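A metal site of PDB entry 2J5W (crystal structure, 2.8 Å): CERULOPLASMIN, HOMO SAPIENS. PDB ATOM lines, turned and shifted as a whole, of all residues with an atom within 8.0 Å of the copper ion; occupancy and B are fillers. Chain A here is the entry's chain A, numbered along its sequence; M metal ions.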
ATOM      1  N   GLU A 291     -17.044  13.387   6.708  1.00  0.00           N
ATOM      2  CA  GLU A 291     -17.325  14.820   6.648  1.00  0.00           C
ATOM      3  C   GLU A 291     -16.747  15.635   7.825  1.00  0.00           C
ATOM      4  O   GLU A 291     -16.473  16.828   7.663  1.00  0.00           O
ATOM      5  CB  GLU A 291     -18.826  15.066   6.543  1.00  0.00           C
ATOM      6  CG  GLU A 291     -19.442  14.632   5.218  1.00  0.00           C
ATOM      7  CD  GLU A 291     -20.967  14.564   5.257  1.00  0.00           C
ATOM      8  OE1 GLU A 291     -21.534  14.531   6.377  1.00  0.00           O
ATOM      9  OE2 GLU A 291     -21.604  14.550   4.184  1.00  0.00           O
ATOM     10  N   PRO A 318     -10.548  13.598   3.834  1.00  0.00           N
ATOM     11  CA  PRO A 318     -10.450  12.165   3.624  1.00  0.00           C
ATOM     12  C   PRO A 318      -9.738  11.776   2.318  1.00  0.00           C
ATOM     13  O   PRO A 318     -10.297  11.910   1.237  1.00  0.00           O
ATOM     14  CB  PRO A 318     -11.907  11.725   3.629  1.00  0.00           C
ATOM     15  CG  PRO A 318     -12.585  12.760   4.475  1.00  0.00           C
ATOM     16  CD  PRO A 318     -11.938  14.019   4.086  1.00  0.00           C
ATOM     17  N   PHE A 920     -19.430  17.125  -8.577  1.00  0.00           N
ATOM     18  CA  PHE A 920     -19.573  16.392  -7.338  1.00  0.00           C
ATOM     19  C   PHE A 920     -20.440  17.241  -6.436  1.00  0.00           C
ATOM     20  O   PHE A 920     -19.991  18.269  -5.944  1.00  0.00           O
ATOM     21  CB  PHE A 920     -18.213  16.078  -6.726  1.00  0.00           C
ATOM     22  CG  PHE A 920     -17.545  14.909  -7.384  1.00  0.00           C
ATOM     23  CD1 PHE A 920     -17.043  15.019  -8.674  1.00  0.00           C
ATOM     24  CD2 PHE A 920     -17.470  13.683  -6.757  1.00  0.00           C
ATOM     25  CE1 PHE A 920     -16.442  13.918  -9.305  1.00  0.00           C
ATOM     26  CE2 PHE A 920     -16.878  12.581  -7.388  1.00  0.00           C
ATOM     27  CZ  PHE A 920     -16.369  12.704  -8.671  1.00  0.00           C
ATOM     28  N   LEU A 921     -21.685  16.825  -6.271  1.00  0.00           N
ATOM     29  CA  LEU A 921     -22.675  17.617  -5.533  1.00  0.00           C
ATOM     30  C   LEU A 921     -23.719  16.709  -4.891  1.00  0.00           C
ATOM     31  O   LEU A 921     -24.304  15.872  -5.543  1.00  0.00           O
ATOM     32  CB  LEU A 921     -23.354  18.631  -6.452  1.00  0.00           C
ATOM     33  CG  LEU A 921     -24.513  19.495  -5.944  1.00  0.00           C
ATOM     34  CD1 LEU A 921     -24.069  20.446  -4.873  1.00  0.00           C
ATOM     35  CD2 LEU A 921     -25.100  20.256  -7.099  1.00  0.00           C
ATOM     36  N   VAL A 922     -23.912  16.879  -3.594  1.00  0.00           N
ATOM     37  CA  VAL A 922     -25.017  16.289  -2.896  1.00  0.00           C
ATOM     38  C   VAL A 922     -26.188  17.167  -3.260  1.00  0.00           C
ATOM     39  O   VAL A 922     -26.287  18.290  -2.763  1.00  0.00           O
ATOM     40  CB  VAL A 922     -24.817  16.322  -1.358  1.00  0.00           C
ATOM     41  CG1 VAL A 922     -26.068  15.816  -0.675  1.00  0.00           C
ATOM     42  CG2 VAL A 922     -23.620  15.505  -0.958  1.00  0.00           C
ATOM     43  N   HIS A 959     -26.458  12.040  -3.095  1.00  0.00           N
ATOM     44  CA  HIS A 959     -25.023  12.139  -3.194  1.00  0.00           C
ATOM     45  C   HIS A 959     -24.580  11.637  -4.562  1.00  0.00           C
ATOM     46  O   HIS A 959     -24.218  10.461  -4.700  1.00  0.00           O
ATOM     47  CB  HIS A 959     -24.398  11.302  -2.080  1.00  0.00           C
ATOM     48  CG  HIS A 959     -24.753  11.764  -0.704  1.00  0.00           C
ATOM     49  ND1 HIS A 959     -26.056  11.855  -0.272  1.00  0.00           N
ATOM     50  CD2 HIS A 959     -23.982  12.148   0.333  1.00  0.00           C
ATOM     51  CE1 HIS A 959     -26.076  12.299   0.977  1.00  0.00           C
ATOM     52  NE2 HIS A 959     -24.824  12.469   1.369  1.00  0.00           N
ATOM     53  N   ALA A 960     -24.595  12.524  -5.551  1.00  0.00           N
ATOM     54  CA  ALA A 960     -24.432  12.125  -6.953  1.00  0.00           C
ATOM     55  C   ALA A 960     -23.190  12.718  -7.605  1.00  0.00           C
ATOM     56  O   ALA A 960     -22.672  13.736  -7.161  1.00  0.00           O
ATOM     57  CB  ALA A 960     -25.672  12.529  -7.760  1.00  0.00           C
ATOM     58  N   ILE A 991     -21.043  20.362   3.852  1.00  0.00           N
ATOM     59  CA  ILE A 991     -20.691  18.953   3.786  1.00  0.00           C
ATOM     60  C   ILE A 991     -20.264  18.511   2.383  1.00  0.00           C
ATOM     61  O   ILE A 991     -19.936  17.345   2.170  1.00  0.00           O
ATOM     62  CB  ILE A 991     -21.839  18.041   4.367  1.00  0.00           C
ATOM     63  CG1 ILE A 991     -23.160  18.186   3.587  1.00  0.00           C
ATOM     64  CG2 ILE A 991     -22.061  18.382   5.834  1.00  0.00           C
ATOM     65  CD1 ILE A 991     -23.112  17.748   2.178  1.00  0.00           C
ATOM     66  N   ASP A 992     -20.240  19.448   1.426  1.00  0.00           N
ATOM     67  CA  ASP A 992     -19.838  19.123   0.052  1.00  0.00           C
ATOM     68  C   ASP A 992     -18.323  19.218  -0.108  1.00  0.00           C
ATOM     69  O   ASP A 992     -17.823  19.860  -1.032  1.00  0.00           O
ATOM     70  CB  ASP A 992     -20.563  20.011  -0.981  1.00  0.00           C
ATOM     71  CG  ASP A 992     -21.945  19.460  -1.365  1.00  0.00           C
ATOM     72  OD1 ASP A 992     -21.982  18.513  -2.169  1.00  0.00           O
ATOM     73  OD2 ASP A 992     -22.992  19.991  -0.886  1.00  0.00           O
ATOM     74  N   LEU A 993     -17.584  18.582   0.791  1.00  0.00           N
ATOM     75  CA  LEU A 993     -16.153  18.436   0.565  1.00  0.00           C
ATOM     76  C   LEU A 993     -16.013  17.077  -0.022  1.00  0.00           C
ATOM     77  O   LEU A 993     -16.378  16.090   0.611  1.00  0.00           O
ATOM     78  CB  LEU A 993     -15.267  18.657   1.813  1.00  0.00           C
ATOM     79  CG  LEU A 993     -15.356  17.995   3.187  1.00  0.00           C
ATOM     80  CD1 LEU A 993     -16.721  18.195   3.805  1.00  0.00           C
ATOM     81  CD2 LEU A 993     -14.901  16.530   3.193  1.00  0.00           C
ATOM     82  N   HIS A 994     -15.497  17.055  -1.239  1.00  0.00           N
ATOM     83  CA  HIS A 994     -15.411  15.856  -2.036  1.00  0.00           C
ATOM     84  C   HIS A 994     -13.978  15.600  -2.459  1.00  0.00           C
ATOM     85  O   HIS A 994     -13.319  16.456  -3.054  1.00  0.00           O
ATOM     86  CB  HIS A 994     -16.295  16.015  -3.250  1.00  0.00           C
ATOM     87  CG  HIS A 994     -17.719  16.281  -2.916  1.00  0.00           C
ATOM     88  ND1 HIS A 994     -18.506  15.393  -2.223  1.00  0.00           N
ATOM     89  CD2 HIS A 994     -18.507  17.356  -3.174  1.00  0.00           C
ATOM     90  CE1 HIS A 994     -19.717  15.900  -2.058  1.00  0.00           C
ATOM     91  NE2 HIS A 994     -19.749  17.084  -2.641  1.00  0.00           N
ATOM     92  N   THR A 995     -13.532  14.381  -2.209  1.00  0.00           N
ATOM     93  CA  THR A 995     -12.158  14.006  -2.394  1.00  0.00           C
ATOM     94  C   THR A 995     -12.120  12.956  -3.514  1.00  0.00           C
ATOM     95  O   THR A 995     -12.229  11.769  -3.280  1.00  0.00           O
ATOM     96  CB  THR A 995     -11.600  13.520  -1.053  1.00  0.00           C
ATOM     97  OG1 THR A 995     -10.480  12.686  -1.277  1.00  0.00           O
ATOM     98  CG2 THR A 995     -12.633  12.725  -0.321  1.00  0.00           C
ATOM     99  N   VAL A 996     -11.955  13.436  -4.742  1.00  0.00           N
ATOM    100  CA  VAL A 996     -12.228  12.648  -5.950  1.00  0.00           C
ATOM    101  C   VAL A 996     -11.079  11.709  -6.259  1.00  0.00           C
ATOM    102  O   VAL A 996      -9.978  12.150  -6.535  1.00  0.00           O
ATOM    103  CB  VAL A 996     -12.477  13.567  -7.167  1.00  0.00           C
ATOM    104  CG1 VAL A 996     -12.806  12.765  -8.391  1.00  0.00           C
ATOM    105  CG2 VAL A 996     -13.605  14.515  -6.868  1.00  0.00           C
ATOM    106  N   ILE A1018     -12.065  18.624  -3.939  1.00  0.00           N
ATOM    107  CA  ILE A1018     -13.023  19.477  -4.601  1.00  0.00           C
ATOM    108  C   ILE A1018     -14.012  20.005  -3.570  1.00  0.00           C
ATOM    109  O   ILE A1018     -14.528  19.239  -2.765  1.00  0.00           O
ATOM    110  CB  ILE A1018     -13.771  18.690  -5.680  1.00  0.00           C
ATOM    111  CG1 ILE A1018     -12.842  18.449  -6.871  1.00  0.00           C
ATOM    112  CG2 ILE A1018     -15.039  19.411  -6.111  1.00  0.00           C
ATOM    113  CD1 ILE A1018     -12.528  19.709  -7.646  1.00  0.00           C
ATOM    114  N   HIS A1039     -14.686   7.470  -7.419  1.00  0.00           N
ATOM    115  CA  HIS A1039     -15.573   7.823  -6.316  1.00  0.00           C
ATOM    116  C   HIS A1039     -14.990   8.893  -5.371  1.00  0.00           C
ATOM    117  O   HIS A1039     -13.794   9.032  -5.237  1.00  0.00           O
ATOM    118  CB  HIS A1039     -15.897   6.555  -5.529  1.00  0.00           C
ATOM    119  CG  HIS A1039     -14.700   5.949  -4.838  1.00  0.00           C
ATOM    120  ND1 HIS A1039     -14.294   6.351  -3.583  1.00  0.00           N
ATOM    121  CD2 HIS A1039     -13.843   4.977  -5.221  1.00  0.00           C
ATOM    122  CE1 HIS A1039     -13.223   5.648  -3.237  1.00  0.00           C
ATOM    123  NE2 HIS A1039     -12.943   4.807  -4.205  1.00  0.00           N
ATOM    124  N   CYS A1040     -15.863   9.655  -4.719  1.00  0.00           N
ATOM    125  CA  CYS A1040     -15.455  10.511  -3.631  1.00  0.00           C
ATOM    126  C   CYS A1040     -15.049   9.575  -2.508  1.00  0.00           C
ATOM    127  O   CYS A1040     -15.656   8.536  -2.344  1.00  0.00           O
ATOM    128  CB  CYS A1040     -16.608  11.398  -3.205  1.00  0.00           C
ATOM    129  SG  CYS A1040     -16.317  12.291  -1.708  1.00  0.00           S
ATOM    130  N   HIS A1041     -14.019   9.949  -1.745  1.00  0.00           N
ATOM    131  CA  HIS A1041     -13.393   9.074  -0.757  1.00  0.00           C
ATOM    132  C   HIS A1041     -13.881   9.394   0.658  1.00  0.00           C
ATOM    133  O   HIS A1041     -13.359   8.850   1.613  1.00  0.00           O
ATOM    134  CB  HIS A1041     -11.871   9.255  -0.839  1.00  0.00           C
ATOM    135  CG  HIS A1041     -11.076   8.046  -0.454  1.00  0.00           C
ATOM    136  ND1 HIS A1041     -10.996   7.581   0.846  1.00  0.00           N
ATOM    137  CD2 HIS A1041     -10.258   7.245  -1.188  1.00  0.00           C
ATOM    138  CE1 HIS A1041     -10.187   6.539   0.880  1.00  0.00           C
ATOM    139  NE2 HIS A1041      -9.727   6.306  -0.334  1.00  0.00           N
ATOM    140  N   VAL A1042     -14.851  10.293   0.809  1.00  0.00           N
ATOM    141  CA  VAL A1042     -15.489  10.550   2.112  1.00  0.00           C
ATOM    142  C   VAL A1042     -16.446   9.392   2.473  1.00  0.00           C
ATOM    143  O   VAL A1042     -17.368   9.091   1.724  1.00  0.00           O
ATOM    144  CB  VAL A1042     -16.344  11.836   2.109  1.00  0.00           C
ATOM    145  CG1 VAL A1042     -16.899  12.092   3.492  1.00  0.00           C
ATOM    146  CG2 VAL A1042     -15.519  13.029   1.604  1.00  0.00           C
ATOM    147  N   THR A1043     -16.235   8.791   3.630  1.00  0.00           N
ATOM    148  CA  THR A1043     -17.051   7.651   4.075  1.00  0.00           C
ATOM    149  C   THR A1043     -18.535   7.813   3.777  1.00  0.00           C
ATOM    150  O   THR A1043     -19.088   7.049   2.996  1.00  0.00           O
ATOM    151  CB  THR A1043     -16.871   7.415   5.568  1.00  0.00           C
ATOM    152  OG1 THR A1043     -15.543   6.952   5.808  1.00  0.00           O
ATOM    153  CG2 THR A1043     -17.876   6.382   6.068  1.00  0.00           C
ATOM    154  N   ASP A1044     -19.157   8.813   4.377  1.00  0.00           N
ATOM    155  CA  ASP A1044     -20.593   9.029   4.284  1.00  0.00           C
ATOM    156  C   ASP A1044     -21.038   9.187   2.815  1.00  0.00           C
ATOM    157  O   ASP A1044     -22.114   8.745   2.447  1.00  0.00           O
ATOM    158  CB  ASP A1044     -20.964  10.217   5.173  1.00  0.00           C
ATOM    159  CG  ASP A1044     -22.409  10.568   5.127  1.00  0.00           C
ATOM    160  OD1 ASP A1044     -22.900  10.960   4.049  1.00  0.00           O
ATOM    161  OD2 ASP A1044     -23.066  10.511   6.185  1.00  0.00           O
ATOM    162  N   HIS A1045     -20.189   9.768   1.955  1.00  0.00           N
ATOM    163  CA  HIS A1045     -20.543   9.950   0.548  1.00  0.00           C
ATOM    164  C   HIS A1045     -20.416   8.678  -0.312  1.00  0.00           C
ATOM    165  O   HIS A1045     -21.181   8.492  -1.259  1.00  0.00           O
ATOM    166  CB  HIS A1045     -19.697  11.044  -0.080  1.00  0.00           C
ATOM    167  CG  HIS A1045     -19.832  12.378   0.582  1.00  0.00           C
ATOM    168  ND1 HIS A1045     -19.058  13.465   0.236  1.00  0.00           N
ATOM    169  CD2 HIS A1045     -20.636  12.791   1.592  1.00  0.00           C
ATOM    170  CE1 HIS A1045     -19.386  14.495   0.986  1.00  0.00           C
ATOM    171  NE2 HIS A1045     -20.340  14.111   1.829  1.00  0.00           N
ATOM    172  N   ILE A1046     -19.437   7.826  -0.014  1.00  0.00           N
ATOM    173  CA  ILE A1046     -19.265   6.559  -0.737  1.00  0.00           C
ATOM    174  C   ILE A1046     -20.495   5.700  -0.493  1.00  0.00           C
ATOM    175  O   ILE A1046     -21.145   5.260  -1.433  1.00  0.00           O
ATOM    176  CB  ILE A1046     -18.038   5.745  -0.257  1.00  0.00           C
ATOM    177  CG1 ILE A1046     -16.741   6.513  -0.423  1.00  0.00           C
ATOM    178  CG2 ILE A1046     -17.914   4.437  -1.039  1.00  0.00           C
ATOM    179  CD1 ILE A1046     -15.538   5.771   0.167  1.00  0.00           C
ATOM    180  N   MET A1050     -22.078   8.157  -3.980  1.00  0.00           N
ATOM    181  CA  MET A1050     -21.344   9.093  -4.808  1.00  0.00           C
ATOM    182  C   MET A1050     -20.144   8.413  -5.495  1.00  0.00           C
ATOM    183  O   MET A1050     -18.989   8.627  -5.126  1.00  0.00           O
ATOM    184  CB  MET A1050     -20.880  10.270  -3.968  1.00  0.00           C
ATOM    185  CG  MET A1050     -20.353  11.440  -4.768  1.00  0.00           C
ATOM    186  SD  MET A1050     -20.082  12.892  -3.740  1.00  0.00           S
ATOM    187  CE  MET A1050     -21.750  13.423  -3.450  1.00  0.00           C
HETATM  188 CU    CU M   1     -17.886  13.710  -1.392  1.00  0.00          CU
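SD of Met 1050 sits close to ND1 of His 994 (3.3 Å).
A ring nitrogen (NE2) of His 994 is in hydrogen-bond range of the side-chain carboxylate of Asp 992 (2.7 Å).
N of Ile 1018 lies within hydrogen-bond range of O of His 994 (2.7 Å).
The backbone carbonyl oxygen (O) of Ile 991 sits close to a ring nitrogen (NE2) of His 1045 (3.3 Å).
A ring nitrogen (NE2) of His 1045 lies within hydrogen-bond range of the side-chain carboxylate (OE2) of Glu 291, at 2.7 Å.
The backbone NH (N) of Cys 1040 is in hydrogen-bond range of the backbone carbonyl oxygen (O) of Met 1050, at 3.3 Å.
The side-chain sulfur (SG) of Cys 1040 lies close to the backbone NH (N) of Val 1042 (3.5 Å).
N of Thr 995 lies close to SG of Cys 1040 (3.5 Å).
Residues that only touch the copper ion: Leu 993, Val 1042 and Met 1050.
Of the 23 residues printed, 6 come within 4 Å of the copper ion.
Along chain A the residues within 4 Å of the copper ion span positions 993 to 1050.
The nearest printed residue that does not touch the copper ion is Thr 995 (4.5 Å).
The copper ion is bound by ND1 of His 994 (2.0 Å), ND1 of His 1045 (2.0 Å) and SG of Cys 1040 (2.1 Å).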
